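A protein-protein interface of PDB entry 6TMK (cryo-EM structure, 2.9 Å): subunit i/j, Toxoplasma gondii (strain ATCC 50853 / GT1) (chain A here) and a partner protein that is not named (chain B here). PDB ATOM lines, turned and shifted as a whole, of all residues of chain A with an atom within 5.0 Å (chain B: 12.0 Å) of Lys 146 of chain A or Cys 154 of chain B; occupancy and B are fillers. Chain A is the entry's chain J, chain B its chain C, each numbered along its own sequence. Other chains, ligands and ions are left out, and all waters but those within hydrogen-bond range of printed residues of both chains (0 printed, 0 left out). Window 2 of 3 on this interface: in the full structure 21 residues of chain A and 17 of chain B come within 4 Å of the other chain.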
ATOM      1  N   ASN A 138     -20.076 -19.686  22.082  1.00  0.00           N
ATOM      2  CA  ASN A 138     -19.891 -18.326  21.587  1.00  0.00           C
ATOM      3  C   ASN A 138     -18.837 -18.390  20.488  1.00  0.00           C
ATOM      4  O   ASN A 138     -17.652 -18.117  20.726  1.00  0.00           O
ATOM      5  CB  ASN A 138     -19.493 -17.383  22.712  1.00  0.00           C
ATOM      6  CG  ASN A 138     -20.562 -17.274  23.766  1.00  0.00           C
ATOM      7  OD1 ASN A 138     -21.493 -16.482  23.654  1.00  0.00           O
ATOM      8  ND2 ASN A 138     -20.449 -18.098  24.787  1.00  0.00           N
ATOM      9  N   LYS A 141     -16.193 -15.266  19.422  1.00  0.00           N
ATOM     10  CA  LYS A 141     -16.030 -14.292  20.481  1.00  0.00           C
ATOM     11  C   LYS A 141     -15.027 -14.792  21.513  1.00  0.00           C
ATOM     12  O   LYS A 141     -14.489 -15.897  21.417  1.00  0.00           O
ATOM     13  CB  LYS A 141     -17.381 -13.980  21.121  1.00  0.00           C
ATOM     14  CG  LYS A 141     -18.350 -13.308  20.170  1.00  0.00           C
ATOM     15  CD  LYS A 141     -19.753 -13.792  20.380  1.00  0.00           C
ATOM     16  CE  LYS A 141     -20.664 -13.365  19.254  1.00  0.00           C
ATOM     17  NZ  LYS A 141     -20.683 -11.898  19.087  1.00  0.00           N
ATOM     18  N   ARG A 142     -14.784 -13.945  22.509  1.00  0.00           N
ATOM     19  CA  ARG A 142     -13.782 -14.181  23.545  1.00  0.00           C
ATOM     20  C   ARG A 142     -14.446 -13.990  24.900  1.00  0.00           C
ATOM     21  O   ARG A 142     -14.646 -12.845  25.337  1.00  0.00           O
ATOM     22  CB  ARG A 142     -12.594 -13.247  23.386  1.00  0.00           C
ATOM     23  CG  ARG A 142     -11.754 -13.526  22.175  1.00  0.00           C
ATOM     24  CD  ARG A 142     -10.619 -12.553  22.057  1.00  0.00           C
ATOM     25  NE  ARG A 142      -9.653 -12.684  23.137  1.00  0.00           N
ATOM     26  CZ  ARG A 142      -8.695 -13.599  23.182  1.00  0.00           C
ATOM     27  NH1 ARG A 142      -7.870 -13.631  24.206  1.00  0.00           N
ATOM     28  NH2 ARG A 142      -8.562 -14.480  22.214  1.00  0.00           N
ATOM     29  N   PRO A 143     -14.806 -15.065  25.584  1.00  0.00           N
ATOM     30  CA  PRO A 143     -15.651 -14.921  26.772  1.00  0.00           C
ATOM     31  C   PRO A 143     -14.905 -14.672  28.071  1.00  0.00           C
ATOM     32  O   PRO A 143     -15.491 -14.824  29.144  1.00  0.00           O
ATOM     33  CB  PRO A 143     -16.398 -16.258  26.809  1.00  0.00           C
ATOM     34  CG  PRO A 143     -15.458 -17.205  26.221  1.00  0.00           C
ATOM     35  CD  PRO A 143     -14.681 -16.476  25.181  1.00  0.00           C
ATOM     36  N   GLY A 144     -13.633 -14.284  28.006  1.00  0.00           N
ATOM     37  CA  GLY A 144     -12.908 -13.988  29.230  1.00  0.00           C
ATOM     38  C   GLY A 144     -13.559 -12.883  30.042  1.00  0.00           C
ATOM     39  O   GLY A 144     -13.638 -12.961  31.270  1.00  0.00           O
ATOM     40  N   LEU A 145     -14.042 -11.843  29.365  1.00  0.00           N
ATOM     41  CA  LEU A 145     -14.635 -10.711  30.060  1.00  0.00           C
ATOM     42  C   LEU A 145     -15.965 -11.085  30.701  1.00  0.00           C
ATOM     43  O   LEU A 145     -16.234 -10.729  31.857  1.00  0.00           O
ATOM     44  CB  LEU A 145     -14.816  -9.566  29.072  1.00  0.00           C
ATOM     45  CG  LEU A 145     -15.165  -8.180  29.589  1.00  0.00           C
ATOM     46  CD1 LEU A 145     -14.120  -7.705  30.545  1.00  0.00           C
ATOM     47  CD2 LEU A 145     -15.280  -7.245  28.436  1.00  0.00           C
ATOM     48  N   LYS A 146     -16.810 -11.807  29.967  1.00  0.00           N
ATOM     49  CA  LYS A 146     -18.061 -12.279  30.535  1.00  0.00           C
ATOM     50  C   LYS A 146     -17.824 -13.255  31.677  1.00  0.00           C
ATOM     51  O   LYS A 146     -18.614 -13.311  32.619  1.00  0.00           O
ATOM     52  CB  LYS A 146     -18.916 -12.915  29.445  1.00  0.00           C
ATOM     53  CG  LYS A 146     -19.225 -12.005  28.296  1.00  0.00           C
ATOM     54  CD  LYS A 146     -19.947 -10.749  28.736  1.00  0.00           C
ATOM     55  CE  LYS A 146     -20.547 -10.009  27.552  1.00  0.00           C
ATOM     56  NZ  LYS A 146     -21.493  -8.941  27.952  1.00  0.00           N
ATOM     57  N   ILE A 147     -16.741 -14.025  31.615  1.00  0.00           N
ATOM     58  CA  ILE A 147     -16.394 -14.919  32.711  1.00  0.00           C
ATOM     59  C   ILE A 147     -15.997 -14.120  33.945  1.00  0.00           C
ATOM     60  O   ILE A 147     -16.384 -14.453  35.072  1.00  0.00           O
ATOM     61  CB  ILE A 147     -15.288 -15.888  32.265  1.00  0.00           C
ATOM     62  CG1 ILE A 147     -15.868 -16.893  31.276  1.00  0.00           C
ATOM     63  CG2 ILE A 147     -14.708 -16.615  33.451  1.00  0.00           C
ATOM     64  CD1 ILE A 147     -14.863 -17.587  30.437  1.00  0.00           C
ATOM     65  N   SER A 148     -15.216 -13.057  33.753  1.00  0.00           N
ATOM     66  CA  SER A 148     -14.882 -12.172  34.863  1.00  0.00           C
ATOM     67  C   SER A 148     -16.144 -11.593  35.485  1.00  0.00           C
ATOM     68  O   SER A 148     -16.263 -11.506  36.713  1.00  0.00           O
ATOM     69  CB  SER A 148     -13.969 -11.052  34.380  1.00  0.00           C
ATOM     70  OG  SER A 148     -12.723 -11.556  33.954  1.00  0.00           O
ATOM     71  N   LEU A 149     -17.097 -11.193  34.649  1.00  0.00           N
ATOM     72  CA  LEU A 149     -18.327 -10.609  35.164  1.00  0.00           C
ATOM     73  C   LEU A 149     -19.193 -11.653  35.858  1.00  0.00           C
ATOM     74  O   LEU A 149     -19.890 -11.333  36.825  1.00  0.00           O
ATOM     75  CB  LEU A 149     -19.086  -9.912  34.036  1.00  0.00           C
ATOM     76  CG  LEU A 149     -18.341  -8.717  33.448  1.00  0.00           C
ATOM     77  CD1 LEU A 149     -18.953  -8.251  32.162  1.00  0.00           C
ATOM     78  CD2 LEU A 149     -18.314  -7.587  34.429  1.00  0.00           C
ATOM     79  N   MET A 150     -19.142 -12.905  35.406  1.00  0.00           N
ATOM     80  CA  MET A 150     -19.853 -13.972  36.096  1.00  0.00           C
ATOM     81  C   MET A 150     -19.237 -14.235  37.461  1.00  0.00           C
ATOM     82  O   MET A 150     -19.951 -14.532  38.422  1.00  0.00           O
ATOM     83  CB  MET A 150     -19.828 -15.250  35.264  1.00  0.00           C
ATOM     84  CG  MET A 150     -20.726 -15.228  34.063  1.00  0.00           C
ATOM     85  SD  MET A 150     -20.350 -16.519  32.869  1.00  0.00           S
ATOM     86  CE  MET A 150     -21.104 -17.916  33.689  1.00  0.00           C
ATOM     87  N   PRO B 150     -23.785 -23.635  34.636  1.00  0.00           N
ATOM     88  CA  PRO B 150     -23.876 -22.403  33.856  1.00  0.00           C
ATOM     89  C   PRO B 150     -22.778 -22.274  32.814  1.00  0.00           C
ATOM     90  O   PRO B 150     -21.687 -22.831  32.938  1.00  0.00           O
ATOM     91  CB  PRO B 150     -23.774 -21.308  34.922  1.00  0.00           C
ATOM     92  CG  PRO B 150     -23.071 -21.922  36.021  1.00  0.00           C
ATOM     93  CD  PRO B 150     -23.467 -23.353  36.042  1.00  0.00           C
ATOM     94  N   VAL B 151     -23.092 -21.501  31.781  1.00  0.00           N
ATOM     95  CA  VAL B 151     -22.210 -21.268  30.650  1.00  0.00           C
ATOM     96  C   VAL B 151     -22.286 -19.794  30.293  1.00  0.00           C
ATOM     97  O   VAL B 151     -23.330 -19.152  30.439  1.00  0.00           O
ATOM     98  CB  VAL B 151     -22.582 -22.163  29.444  1.00  0.00           C
ATOM     99  CG1 VAL B 151     -21.857 -21.727  28.193  1.00  0.00           C
ATOM    100  CG2 VAL B 151     -22.252 -23.592  29.743  1.00  0.00           C
ATOM    101  N   ALA B 152     -21.166 -19.256  29.833  1.00  0.00           N
ATOM    102  CA  ALA B 152     -21.097 -17.843  29.517  1.00  0.00           C
ATOM    103  C   ALA B 152     -21.748 -17.550  28.170  1.00  0.00           C
ATOM    104  O   ALA B 152     -21.869 -18.413  27.301  1.00  0.00           O
ATOM    105  CB  ALA B 152     -19.645 -17.367  29.506  1.00  0.00           C
ATOM    106  N   TRP B 153     -22.161 -16.295  28.015  1.00  0.00           N
ATOM    107  CA  TRP B 153     -22.819 -15.789  26.820  1.00  0.00           C
ATOM    108  C   TRP B 153     -22.168 -14.481  26.411  1.00  0.00           C
ATOM    109  O   TRP B 153     -22.044 -13.562  27.228  1.00  0.00           O
ATOM    110  CB  TRP B 153     -24.308 -15.590  27.063  1.00  0.00           C
ATOM    111  CG  TRP B 153     -25.141 -15.567  25.834  1.00  0.00           C
ATOM    112  CD1 TRP B 153     -24.853 -14.956  24.657  1.00  0.00           C
ATOM    113  CD2 TRP B 153     -26.412 -16.186  25.660  1.00  0.00           C
ATOM    114  NE1 TRP B 153     -25.867 -15.150  23.762  1.00  0.00           N
ATOM    115  CE2 TRP B 153     -26.837 -15.909  24.353  1.00  0.00           C
ATOM    116  CE3 TRP B 153     -27.232 -16.954  26.485  1.00  0.00           C
ATOM    117  CZ2 TRP B 153     -28.044 -16.369  23.855  1.00  0.00           C
ATOM    118  CZ3 TRP B 153     -28.419 -17.403  25.991  1.00  0.00           C
ATOM    119  CH2 TRP B 153     -28.819 -17.112  24.689  1.00  0.00           C
ATOM    120  N   CYS B 154     -21.774 -14.395  25.148  1.00  0.00           N
ATOM    121  CA  CYS B 154     -21.256 -13.160  24.588  1.00  0.00           C
ATOM    122  C   CYS B 154     -22.049 -12.741  23.355  1.00  0.00           C
ATOM    123  O   CYS B 154     -21.590 -11.918  22.561  1.00  0.00           O
ATOM    124  CB  CYS B 154     -19.792 -13.333  24.216  1.00  0.00           C
ATOM    125  SG  CYS B 154     -18.784 -14.026  25.522  1.00  0.00           S
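The backbone carbonyl oxygen (O) of Ala 152 of chain B lies within hydrogen-bond range of the side-chain amide nitrogen (ND2) of Asn 138 of chain A, 2.9 Å away.
N of Cys 154 of chain B sits at hydrogen-bond distance from OD1 of Asn 138 of chain A, at 2.6 Å.
Asn 138 of chain A touches Trp 153 of chain B (OD1 to C, 3.5 Å).
Lys 141 of chain A touches Cys 154 of chain B (CD to O, 3.4 Å).
CA of Pro 143 of chain A touches SG of Cys 154 of chain B, at 3.5 Å.
Lys 146 of chain A touches Trp 153 of chain B (CG to O, 3.4 Å).
Lys 146 of chain A touches Cys 154 of chain B.
Ala 152 of chain B touches Met 150 of chain A.
Lys 141 of chain A touches just one residue of chain B: Cys 154 (3.4 Å).
Arg 142 of chain A touches none of the printed residues of chain B.
Gly 144 of chain A touches none of the printed residues of chain B.
No residue of chain B comes within 4 Å of Leu 145 of chain A.
Of the printed residues of chain B, Lys 146 of chain A touches Trp 153 and Cys 154.
No residue of chain B comes within 4 Å of Ile 147 of chain A.
Ser 148 of chain A touches none of the printed residues of chain B.
Pro 150 of chain B touches none of the printed residues of chain A.
Printed residues of chain A within 4 Å of Ala 152 of chain B: Asn 138 and Met 150.
Printed residues of chain A within 4 Å of Trp 153 of chain B: Asn 138 (3.5 Å) and Lys 146 (3.4 Å).
Of the printed residues of chain A, Cys 154 of chain B touches Asn 138 (2.6 Å), Lys 141 (3.4 Å), Pro 143 (3.5 Å) and Lys 146 (3.5 Å).
The nearest residue of chain A that does not touch Cys 154 of chain B is Arg 142 of chain A (4.3 Å).
The nearest printed residue of chain A that does not touch Ala 152 of chain B is Ile 147 of chain A (4.2 Å).
Along chain B the printed residues that touch a printed residue of chain A span positions 152 to 154.
Hydrophobic or aromatic side chains of chain A that line the printed part of chain B: Pro 143 and Met 150.
Among the printed residues, 8 pairs touch across the chains.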
